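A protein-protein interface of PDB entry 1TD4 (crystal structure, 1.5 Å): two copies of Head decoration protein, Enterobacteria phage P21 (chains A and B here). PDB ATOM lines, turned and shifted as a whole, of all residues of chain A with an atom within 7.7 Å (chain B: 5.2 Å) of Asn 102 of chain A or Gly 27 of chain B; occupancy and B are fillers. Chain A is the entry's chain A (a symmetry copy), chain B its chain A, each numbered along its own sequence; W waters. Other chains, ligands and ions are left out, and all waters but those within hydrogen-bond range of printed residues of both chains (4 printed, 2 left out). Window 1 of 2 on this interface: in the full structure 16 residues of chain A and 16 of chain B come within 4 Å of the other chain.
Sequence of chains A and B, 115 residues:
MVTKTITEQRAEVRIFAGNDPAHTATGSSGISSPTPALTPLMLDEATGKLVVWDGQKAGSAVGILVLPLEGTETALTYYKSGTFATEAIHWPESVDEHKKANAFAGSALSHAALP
O of Gly 27 of chain B is in hydrogen-bond range of N of Leu 76 of chain B (2.9 Å). The backbone carbonyl oxygen (O) of Ser 28 of chain B lies within hydrogen-bond range of the backbone NH (N) of Leu 50 of chain B (2.9 Å). N of Gly 59 of chain A lies within hydrogen-bond range of O of Asn 102 of chain A (3.0 Å). N of Gly 59 of chain A is in hydrogen-bond range of O of Ala 103 of chain A (3.0 Å). The backbone NH (N) of Lys 99 of chain A is in hydrogen-bond range of the side-chain carboxylate (OD2) of Asp 96 of chain A (2.9 Å). A ring nitrogen (NE2) of His 111 of chain A lies within hydrogen-bond range of the backbone carbonyl oxygen (O) of Ala 101 of chain A, 3.3 Å away.
N of Ser 28 of chain B lies within hydrogen-bond range of OD1 of Asn 102 of chain A (3.0 Å). ND2 of Asn 102 of chain A is in hydrogen-bond range of O of Gly 48 of chain B, 2.8 Å away.
No position is printed for both chains.
Of the 21 printed residues of chain A, 9 touch a printed residue of chain B. Hydrophobic or aromatic side chains of chain A that line the printed part of chain B: Ala 58, His 98, Ala 101 and Ala 105. Along chain A the printed residues that touch a printed residue of chain B span positions 58 to 111. Of the 13 printed residues of chain B, 9 touch a printed residue of chain A. Among the printed residues, no Asp or Glu carboxylate lies within 4 Å of a Lys or Arg side-chain nitrogen of the other chain.
Water W3 bridges OH of Tyr 78 of chain B and O of Leu 109 of chain A. Water W1 bridges O of Thr 26 of chain B (2.8 Å) and N of His 111 of chain A (3.0 Å). Water W2 lies within hydrogen-bond range of O of His 111 of chain A (2.9 Å) and N of Thr 26 of chain B (3.0 Å). Water W4 lies within hydrogen-bond range of the backbone carbonyl oxygen (O) of Leu 109 of chain A (3.1 Å) and the side-chain hydroxyl (OH) of Tyr 78 of chain B (3.4 Å).
Gly 48 of chain B touches Ala 58 of chain A. CD2 of His 98 of chain A touches OG of Ser 28 of chain B, at 3.2 Å. His 98 of chain A touches Gly 48 of chain B (O to O, 3.8 Å). Lys 49 of chain B touches His 98 of chain A (CE to ND1, 3.6 Å). Lys 99 of chain A touches Gly 48 of chain B. CB of Ala 101 of chain A touches CB of Ser 28 of chain B, 3.8 Å away. Gly 27 of chain B touches Asn 102 of chain A (CA to OD1, 3.0 Å). Leu 43 of chain B touches Asn 102 of chain A (CD2 to CB, 3.9 Å). Asn 102 of chain A touches Leu 50 of chain B (ND2 to N, 3.6 Å). CB of Ala 105 of chain A touches OH of Tyr 78 of chain B (3.7 Å).
Of the printed residues of chain B, Asn 102 of chain A touches Gly 27 (3.0 Å), Ser 28 (3.0 Å), Leu 43 (3.9 Å), Gly 48 (2.8 Å), Lys 49 (3.6 Å) and Leu 50 (3.6 Å). Of the printed residues of chain A, Gly 27 of chain B touches Asn 102 (3.0 Å). Of the printed residues of chain B, Gly 59 of chain A touches Leu 43. Of the printed residues of chain B, Ser 110 of chain A touches Ala 25 (3.5 Å). Of the printed residues of chain B, Ala 58 of chain A touches Leu 43 (3.5 Å) and Gly 48 (3.5 Å). The nearest printed residue of chain A that does not touch Gly 48 of chain B is Asp 96 of chain A (5.8 Å).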
ATOM      1  N   TRP A  53      15.803   0.752  13.223  1.00  0.00           N
ATOM      2  CA  TRP A  53      17.104   0.436  12.613  1.00  0.00           C
ATOM      3  C   TRP A  53      17.360   1.319  11.389  1.00  0.00           C
ATOM      4  O   TRP A  53      16.497   1.375  10.507  1.00  0.00           O
ATOM      5  CB  TRP A  53      17.209  -1.030  12.196  1.00  0.00           C
ATOM      6  CG  TRP A  53      18.517  -1.488  11.628  1.00  0.00           C
ATOM      7  CD1 TRP A  53      19.762  -1.527  12.150  1.00  0.00           C
ATOM      8  CD2 TRP A  53      18.750  -2.058  10.330  1.00  0.00           C
ATOM      9  NE1 TRP A  53      20.764  -2.008  11.360  1.00  0.00           N
ATOM     10  CE2 TRP A  53      20.124  -2.362  10.205  1.00  0.00           C
ATOM     11  CE3 TRP A  53      17.867  -2.323   9.280  1.00  0.00           C
ATOM     12  CZ2 TRP A  53      20.652  -2.917   9.063  1.00  0.00           C
ATOM     13  CZ3 TRP A  53      18.414  -2.886   8.131  1.00  0.00           C
ATOM     14  CH2 TRP A  53      19.775  -3.168   8.050  1.00  0.00           C
ATOM     15  N   LYS A  57      24.562  -0.278   9.755  1.00  0.00           N
ATOM     16  CA  LYS A  57      25.435  -1.377  10.122  1.00  0.00           C
ATOM     17  C   LYS A  57      24.703  -2.715  10.182  1.00  0.00           C
ATOM     18  O   LYS A  57      23.634  -2.847  10.780  1.00  0.00           O
ATOM     19  CB  LYS A  57      26.077  -1.150  11.490  1.00  0.00           C
ATOM     20  CG  LYS A  57      27.058   0.030  11.546  1.00  0.00           C
ATOM     21  CD  LYS A  57      27.777  -0.073  12.893  1.00  0.00           C
ATOM     22  CE  LYS A  57      27.589  -1.507  13.384  1.00  0.00           C
ATOM     23  NZ  LYS A  57      28.748  -1.947  14.226  1.00  0.00           N
ATOM     24  N   ALA A  58      25.352  -3.692   9.537  1.00  0.00           N
ATOM     25  CA  ALA A  58      24.920  -5.068   9.747  1.00  0.00           C
ATOM     26  C   ALA A  58      25.032  -5.431  11.214  1.00  0.00           C
ATOM     27  O   ALA A  58      25.966  -5.023  11.922  1.00  0.00           O
ATOM     28  CB  ALA A  58      25.775  -6.044   8.947  1.00  0.00           C
ATOM     29  N   GLY A  59      24.095  -6.271  11.696  1.00  0.00           N
ATOM     30  CA  GLY A  59      24.203  -6.817  13.047  1.00  0.00           C
ATOM     31  C   GLY A  59      23.647  -5.870  14.090  1.00  0.00           C
ATOM     32  O   GLY A  59      23.560  -6.283  15.262  1.00  0.00           O
ATOM     33  N   SER A  60      23.270  -4.642  13.748  1.00  0.00           N
ATOM     34  CA  SER A  60      22.813  -3.717  14.788  1.00  0.00           C
ATOM     35  C   SER A  60      21.285  -3.742  14.900  1.00  0.00           C
ATOM     36  O   SER A  60      20.686  -3.048  15.766  1.00  0.00           O
ATOM     37  CB  SER A  60      23.300  -2.294  14.510  1.00  0.00           C
ATOM     38  OG  SER A  60      22.633  -1.806  13.361  1.00  0.00           O
ATOM     39  N   ALA A  61      20.593  -4.516  14.053  1.00  0.00           N
ATOM     40  CA  ALA A  61      19.127  -4.672  14.220  1.00  0.00           C
ATOM     41  C   ALA A  61      18.929  -5.759  15.283  1.00  0.00           C
ATOM     42  O   ALA A  61      19.306  -6.914  15.046  1.00  0.00           O
ATOM     43  CB  ALA A  61      18.415  -5.039  12.960  1.00  0.00           C
ATOM     44  N   TRP A  91      11.658  -2.606   5.613  1.00  0.00           N
ATOM     45  CA  TRP A  91      13.052  -2.185   5.619  1.00  0.00           C
ATOM     46  C   TRP A  91      13.223  -0.674   5.499  1.00  0.00           C
ATOM     47  O   TRP A  91      12.398  -0.006   4.891  1.00  0.00           O
ATOM     48  CB  TRP A  91      13.778  -2.872   4.456  1.00  0.00           C
ATOM     49  CG  TRP A  91      13.788  -4.368   4.577  1.00  0.00           C
ATOM     50  CD1 TRP A  91      13.064  -5.292   3.872  1.00  0.00           C
ATOM     51  CD2 TRP A  91      14.593  -5.112   5.487  1.00  0.00           C
ATOM     52  NE1 TRP A  91      13.359  -6.591   4.281  1.00  0.00           N
ATOM     53  CE2 TRP A  91      14.311  -6.483   5.287  1.00  0.00           C
ATOM     54  CE3 TRP A  91      15.527  -4.737   6.465  1.00  0.00           C
ATOM     55  CZ2 TRP A  91      14.945  -7.470   6.037  1.00  0.00           C
ATOM     56  CZ3 TRP A  91      16.158  -5.732   7.203  1.00  0.00           C
ATOM     57  CH2 TRP A  91      15.860  -7.091   6.979  1.00  0.00           C
ATOM     58  N   ASP A  96      21.553  -0.994   2.249  1.00  0.00           N
ATOM     59  CA  ASP A  96      22.556  -1.781   1.568  1.00  0.00           C
ATOM     60  C   ASP A  96      22.132  -3.245   1.534  1.00  0.00           C
ATOM     61  O   ASP A  96      21.690  -3.763   2.560  1.00  0.00           O
ATOM     62  CB  ASP A  96      23.873  -1.554   2.330  1.00  0.00           C
ATOM     63  CG  ASP A  96      24.995  -2.387   1.759  1.00  0.00           C
ATOM     64  OD1 ASP A  96      25.886  -1.778   1.136  1.00  0.00           O
ATOM     65  OD2 ASP A  96      24.940  -3.609   1.975  1.00  0.00           O
ATOM     66  N   GLU A  97      22.206  -3.898   0.388  1.00  0.00           N
ATOM     67  CA  GLU A  97      21.718  -5.275   0.257  1.00  0.00           C
ATOM     68  C   GLU A  97      22.427  -6.248   1.177  1.00  0.00           C
ATOM     69  O   GLU A  97      21.780  -7.198   1.685  1.00  0.00           O
ATOM     70  CB  GLU A  97      21.838  -5.710  -1.217  1.00  0.00           C
ATOM     71  CG  GLU A  97      20.959  -4.867  -2.124  1.00  0.00           C
ATOM     72  CD  GLU A  97      19.470  -4.828  -1.884  1.00  0.00           C
ATOM     73  OE1 GLU A  97      18.860  -3.768  -2.198  1.00  0.00           O
ATOM     74  OE2 GLU A  97      18.832  -5.799  -1.403  1.00  0.00           O
ATOM     75  N   HIS A  98      23.718  -6.034   1.429  1.00  0.00           N
ATOM     76  CA  HIS A  98      24.442  -6.943   2.335  1.00  0.00           C
ATOM     77  C   HIS A  98      24.116  -6.670   3.790  1.00  0.00           C
ATOM     78  O   HIS A  98      23.924  -7.590   4.595  1.00  0.00           O
ATOM     79  CB  HIS A  98      25.951  -6.766   2.056  1.00  0.00           C
ATOM     80  CG  HIS A  98      26.238  -6.865   0.587  1.00  0.00           C
ATOM     81  ND1 HIS A  98      26.964  -5.914  -0.104  1.00  0.00           N
ATOM     82  CD2 HIS A  98      25.851  -7.777  -0.339  1.00  0.00           C
ATOM     83  CE1 HIS A  98      27.044  -6.229  -1.383  1.00  0.00           C
ATOM     84  NE2 HIS A  98      26.376  -7.353  -1.553  1.00  0.00           N
ATOM     85  N   LYS A  99      24.045  -5.387   4.142  1.00  0.00           N
ATOM     86  CA  LYS A  99      23.700  -4.999   5.517  1.00  0.00           C
ATOM     87  C   LYS A  99      22.272  -5.432   5.814  1.00  0.00           C
ATOM     88  O   LYS A  99      21.970  -5.811   6.952  1.00  0.00           O
ATOM     89  CB  LYS A  99      23.914  -3.482   5.693  1.00  0.00           C
ATOM     90  CG  LYS A  99      25.389  -3.135   5.559  1.00  0.00           C
ATOM     91  CD  LYS A  99      25.684  -1.662   5.818  1.00  0.00           C
ATOM     92  CE  LYS A  99      27.192  -1.413   5.651  1.00  0.00           C
ATOM     93  NZ  LYS A  99      27.526   0.002   5.957  1.00  0.00           N
ATOM     94  N   LYS A 100      21.403  -5.404   4.812  1.00  0.00           N
ATOM     95  CA  LYS A 100      20.031  -5.903   4.937  1.00  0.00           C
ATOM     96  C   LYS A 100      20.070  -7.413   5.160  1.00  0.00           C
ATOM     97  O   LYS A 100      19.457  -7.894   6.133  1.00  0.00           O
ATOM     98  CB  LYS A 100      19.248  -5.518   3.674  1.00  0.00           C
ATOM     99  CG  LYS A 100      17.948  -6.296   3.471  1.00  0.00           C
ATOM    100  CD  LYS A 100      17.246  -5.691   2.254  1.00  0.00           C
ATOM    101  CE  LYS A 100      15.988  -6.382   1.844  1.00  0.00           C
ATOM    102  NZ  LYS A 100      15.331  -5.797   0.621  1.00  0.00           N
ATOM    103  N   ALA A 101      20.785  -8.176   4.328  1.00  0.00           N
ATOM    104  CA  ALA A 101      20.869  -9.618   4.499  1.00  0.00           C
ATOM    105  C   ALA A 101      21.312  -9.976   5.916  1.00  0.00           C
ATOM    106  O   ALA A 101      20.789 -10.939   6.493  1.00  0.00           O
ATOM    107  CB  ALA A 101      21.869 -10.223   3.490  1.00  0.00           C
ATOM    108  N   ASN A 102      22.284  -9.195   6.432  1.00  0.00           N
ATOM    109  CA  ASN A 102      22.906  -9.503   7.727  1.00  0.00           C
ATOM    110  C   ASN A 102      22.456  -8.543   8.836  1.00  0.00           C
ATOM    111  O   ASN A 102      23.166  -8.374   9.843  1.00  0.00           O
ATOM    112  CB  ASN A 102      24.431  -9.478   7.598  1.00  0.00           C
ATOM    113  CG  ASN A 102      24.903 -10.573   6.635  1.00  0.00           C
ATOM    114  OD1 ASN A 102      24.217 -11.590   6.418  1.00  0.00           O
ATOM    115  ND2 ASN A 102      26.088 -10.321   6.067  1.00  0.00           N
ATOM    116  N   ALA A 103      21.285  -7.930   8.678  1.00  0.00           N
ATOM    117  CA  ALA A 103      20.758  -6.977   9.649  1.00  0.00           C
ATOM    118  C   ALA A 103      20.792  -7.507  11.075  1.00  0.00           C
ATOM    119  O   ALA A 103      21.185  -6.762  11.991  1.00  0.00           O
ATOM    120  CB  ALA A 103      19.328  -6.577   9.287  1.00  0.00           C
ATOM    121  N   PHE A 104      20.399  -8.753  11.253  1.00  0.00           N
ATOM    122  CA  PHE A 104      20.185  -9.316  12.573  1.00  0.00           C
ATOM    123  C   PHE A 104      21.283 -10.272  13.003  1.00  0.00           C
ATOM    124  O   PHE A 104      21.109 -10.906  14.043  1.00  0.00           O
ATOM    125  CB  PHE A 104      18.862 -10.123  12.588  1.00  0.00           C
ATOM    126  CG  PHE A 104      17.668  -9.329  12.063  1.00  0.00           C
ATOM    127  CD1 PHE A 104      17.096  -9.627  10.838  1.00  0.00           C
ATOM    128  CD2 PHE A 104      17.126  -8.294  12.798  1.00  0.00           C
ATOM    129  CE1 PHE A 104      16.027  -8.936  10.326  1.00  0.00           C
ATOM    130  CE2 PHE A 104      16.032  -7.608  12.299  1.00  0.00           C
ATOM    131  CZ  PHE A 104      15.457  -7.916  11.095  1.00  0.00           C
ATOM    132  N   ALA A 105      22.362 -10.407  12.221  1.00  0.00           N
ATOM    133  CA  ALA A 105      23.394 -11.366  12.511  1.00  0.00           C
ATOM    134  C   ALA A 105      23.976 -11.112  13.895  1.00  0.00           C
ATOM    135  O   ALA A 105      24.377  -9.991  14.168  1.00  0.00           O
ATOM    136  CB  ALA A 105      24.519 -11.342  11.473  1.00  0.00           C
ATOM    137  N   GLY A 106      24.021 -12.172  14.704  1.00  0.00           N
ATOM    138  CA  GLY A 106      24.488 -12.090  16.064  1.00  0.00           C
ATOM    139  C   GLY A 106      23.329 -12.202  17.052  1.00  0.00           C
ATOM    140  O   GLY A 106      23.610 -12.533  18.210  1.00  0.00           O
ATOM    141  N   LEU A 109      17.489 -13.733  15.611  1.00  0.00           N
ATOM    142  CA  LEU A 109      16.652 -13.465  14.458  1.00  0.00           C
ATOM    143  C   LEU A 109      17.405 -13.716  13.149  1.00  0.00           C
ATOM    144  O   LEU A 109      18.630 -13.533  13.119  1.00  0.00           O
ATOM    145  CB  LEU A 109      16.182 -12.007  14.390  1.00  0.00           C
ATOM    146  CG  LEU A 109      15.358 -11.570  15.606  1.00  0.00           C
ATOM    147  CD1 LEU A 109      15.590 -10.079  15.880  1.00  0.00           C
ATOM    148  CD2 LEU A 109      13.894 -11.860  15.352  1.00  0.00           C
ATOM    149  N   SER A 110      16.659 -14.033  12.104  1.00  0.00           N
ATOM    150  CA  SER A 110      17.226 -14.122  10.758  1.00  0.00           C
ATOM    151  C   SER A 110      16.070 -13.920   9.787  1.00  0.00           C
ATOM    152  O   SER A 110      14.908 -13.862  10.215  1.00  0.00           O
ATOM    153  CB  SER A 110      17.852 -15.469  10.512  1.00  0.00           C
ATOM    154  OG  SER A 110      16.962 -16.526  10.866  1.00  0.00           O
ATOM    155  N   HIS A 111      16.424 -13.859   8.502  1.00  0.00           N
ATOM    156  CA  HIS A 111      15.370 -13.722   7.500  1.00  0.00           C
ATOM    157  C   HIS A 111      15.856 -14.334   6.197  1.00  0.00           C
ATOM    158  O   HIS A 111      17.072 -14.466   5.983  1.00  0.00           O
ATOM    159  CB  HIS A 111      14.964 -12.247   7.380  1.00  0.00           C
ATOM    160  CG  HIS A 111      15.969 -11.378   6.678  1.00  0.00           C
ATOM    161  ND1 HIS A 111      15.940 -11.075   5.326  1.00  0.00           N
ATOM    162  CD2 HIS A 111      17.029 -10.694   7.217  1.00  0.00           C
ATOM    163  CE1 HIS A 111      16.940 -10.265   5.034  1.00  0.00           C
ATOM    164  NE2 HIS A 111      17.626 -10.033   6.163  1.00  0.00           N
ATOM    165  N   ALA B  25      20.742 -20.101   9.507  1.00  0.00           N
ATOM    166  CA  ALA B  25      20.326 -18.841   8.891  1.00  0.00           C
ATOM    167  C   ALA B  25      21.162 -18.628   7.625  1.00  0.00           C
ATOM    168  O   ALA B  25      22.195 -19.264   7.493  1.00  0.00           O
ATOM    169  CB  ALA B  25      20.542 -17.655   9.825  1.00  0.00           C
ATOM    170  N   THR B  26      20.709 -17.766   6.741  1.00  0.00           N
ATOM    171  CA  THR B  26      21.560 -17.441   5.595  1.00  0.00           C
ATOM    172  C   THR B  26      21.927 -15.969   5.728  1.00  0.00           C
ATOM    173  O   THR B  26      21.261 -15.158   6.411  1.00  0.00           O
ATOM    174  CB  THR B  26      20.863 -17.714   4.266  1.00  0.00           C
ATOM    175  OG1 THR B  26      19.624 -17.004   4.254  1.00  0.00           O
ATOM    176  CG2 THR B  26      20.548 -19.201   4.160  1.00  0.00           C
ATOM    177  N   GLY B  27      23.012 -15.620   5.065  1.00  0.00           N
ATOM    178  CA  GLY B  27      23.582 -14.272   5.181  1.00  0.00           C
ATOM    179  C   GLY B  27      24.448 -14.018   3.955  1.00  0.00           C
ATOM    180  O   GLY B  27      24.799 -14.940   3.199  1.00  0.00           O
ATOM    181  N   SER B  28      24.778 -12.749   3.763  1.00  0.00           N
ATOM    182  CA  SER B  28      25.639 -12.337   2.659  1.00  0.00           C
ATOM    183  C   SER B  28      27.090 -12.633   3.018  1.00  0.00           C
ATOM    184  O   SER B  28      27.544 -12.294   4.130  1.00  0.00           O
ATOM    185  CB  SER B  28      25.448 -10.847   2.405  1.00  0.00           C
ATOM    186  OG  SER B  28      26.450 -10.311   1.572  1.00  0.00           O
ATOM    187  N   SER B  29      27.816 -13.267   2.110  1.00  0.00           N
ATOM    188  CA  SER B  29      29.175 -13.711   2.383  1.00  0.00           C
ATOM    189  C   SER B  29      30.213 -12.753   1.817  1.00  0.00           C
ATOM    190  O   SER B  29      30.107 -12.348   0.655  1.00  0.00           O
ATOM    191  CB  SER B  29      29.407 -15.123   1.789  1.00  0.00           C
ATOM    192  OG  SER B  29      30.769 -15.516   2.023  1.00  0.00           O
ATOM    193  N   LEU B  43      31.119 -10.213  11.492  1.00  0.00           N
ATOM    194  CA  LEU B  43      30.761  -9.246  10.461  1.00  0.00           C
ATOM    195  C   LEU B  43      31.970  -8.393  10.072  1.00  0.00           C
ATOM    196  O   LEU B  43      32.771  -8.059  10.942  1.00  0.00           O
ATOM    197  CB  LEU B  43      29.610  -8.307  10.900  1.00  0.00           C
ATOM    198  CG  LEU B  43      28.283  -9.057  11.076  1.00  0.00           C
ATOM    199  CD1 LEU B  43      27.322  -8.275  11.971  1.00  0.00           C
ATOM    200  CD2 LEU B  43      27.640  -9.352   9.726  1.00  0.00           C
ATOM    201  N   GLY B  48      29.541  -5.038   5.627  1.00  0.00           N
ATOM    202  CA  GLY B  48      28.369  -5.653   6.217  1.00  0.00           C
ATOM    203  C   GLY B  48      28.281  -7.155   5.974  1.00  0.00           C
ATOM    204  O   GLY B  48      27.309  -7.812   6.372  1.00  0.00           O
ATOM    205  N   LYS B  49      29.285  -7.701   5.286  1.00  0.00           N
ATOM    206  CA  LYS B  49      29.247  -9.123   4.939  1.00  0.00           C
ATOM    207  C   LYS B  49      29.845  -9.981   6.016  1.00  0.00           C
ATOM    208  O   LYS B  49      30.584  -9.551   6.925  1.00  0.00           O
ATOM    209  CB  LYS B  49      30.046  -9.354   3.649  1.00  0.00           C
ATOM    210  CG  LYS B  49      29.519  -8.550   2.454  1.00  0.00           C
ATOM    211  CD  LYS B  49      30.417  -8.737   1.236  1.00  0.00           C
ATOM    212  CE  LYS B  49      29.791  -8.070   0.019  1.00  0.00           C
ATOM    213  NZ  LYS B  49      30.608  -8.225  -1.234  1.00  0.00           N
ATOM    214  N   LEU B  50      29.528 -11.276   5.963  1.00  0.00           N
ATOM    215  CA  LEU B  50      30.089 -12.230   6.903  1.00  0.00           C
ATOM    216  C   LEU B  50      31.437 -12.765   6.428  1.00  0.00           C
ATOM    217  O   LEU B  50      31.555 -13.179   5.267  1.00  0.00           O
ATOM    218  CB  LEU B  50      29.064 -13.360   7.093  1.00  0.00           C
ATOM    219  CG  LEU B  50      27.837 -13.007   7.946  1.00  0.00           C
ATOM    220  CD1 LEU B  50      26.726 -13.999   7.654  1.00  0.00           C
ATOM    221  CD2 LEU B  50      28.198 -13.005   9.412  1.00  0.00           C
ATOM    222  N   THR B  74      27.950 -15.837  -3.010  1.00  0.00           N
ATOM    223  CA  THR B  74      27.491 -14.525  -2.500  1.00  0.00           C
ATOM    224  C   THR B  74      26.743 -14.765  -1.196  1.00  0.00           C
ATOM    225  O   THR B  74      26.649 -13.843  -0.375  1.00  0.00           O
ATOM    226  CB  THR B  74      26.624 -13.760  -3.505  1.00  0.00           C
ATOM    227  OG1 THR B  74      25.491 -14.546  -3.917  1.00  0.00           O
ATOM    228  CG2 THR B  74      27.393 -13.441  -4.791  1.00  0.00           C
ATOM    229  N   ALA B  75      26.224 -15.972  -0.935  1.00  0.00           N
ATOM    230  CA  ALA B  75      25.508 -16.185   0.334  1.00  0.00           C
ATOM    231  C   ALA B  75      26.086 -17.391   1.053  1.00  0.00           C
ATOM    232  O   ALA B  75      26.665 -18.236   0.350  1.00  0.00           O
ATOM    233  CB  ALA B  75      24.028 -16.372   0.093  1.00  0.00           C
ATOM    234  N   LEU B  76      25.895 -17.435   2.360  1.00  0.00           N
ATOM    235  CA  LEU B  76      26.343 -18.643   3.080  1.00  0.00           C
ATOM    236  C   LEU B  76      25.245 -19.051   4.059  1.00  0.00           C
ATOM    237  O   LEU B  76      24.347 -18.254   4.334  1.00  0.00           O
ATOM    238  CB  LEU B  76      27.686 -18.367   3.747  1.00  0.00           C
ATOM    239  CG  LEU B  76      27.848 -17.158   4.665  1.00  0.00           C
ATOM    240  CD1 LEU B  76      27.201 -17.352   6.033  1.00  0.00           C
ATOM    241  CD2 LEU B  76      29.331 -16.823   4.939  1.00  0.00           C
ATOM    242  N   TYR B  78      24.715 -20.401   8.000  1.00  0.00           N
ATOM    243  CA  TYR B  78      25.398 -20.498   9.295  1.00  0.00           C
ATOM    244  C   TYR B  78      24.448 -20.925  10.405  1.00  0.00           C
ATOM    245  O   TYR B  78      23.259 -20.717  10.372  1.00  0.00           O
ATOM    246  CB  TYR B  78      26.051 -19.181   9.651  1.00  0.00           C
ATOM    247  CG  TYR B  78      25.215 -17.932   9.790  1.00  0.00           C
ATOM    248  CD1 TYR B  78      24.783 -17.198   8.701  1.00  0.00           C
ATOM    249  CD2 TYR B  78      24.872 -17.471  11.058  1.00  0.00           C
ATOM    250  CE1 TYR B  78      24.018 -16.048   8.862  1.00  0.00           C
ATOM    251  CE2 TYR B  78      24.113 -16.322  11.237  1.00  0.00           C
ATOM    252  CZ  TYR B  78      23.685 -15.614  10.122  1.00  0.00           C
ATOM    253  OH  TYR B  78      22.943 -14.468  10.306  1.00  0.00           O
HETATM  254  O   HOH W   1      19.383 -13.926   8.154  1.00  0.00           O
HETATM  255  O   HOH W   2      17.929 -16.886   7.294  1.00  0.00           O
HETATM  256  O   HOH W   3      20.489 -13.450  10.921  1.00  0.00           O
HETATM  257  O   HOH W   4      21.603 -14.491  13.430  1.00  0.00           O
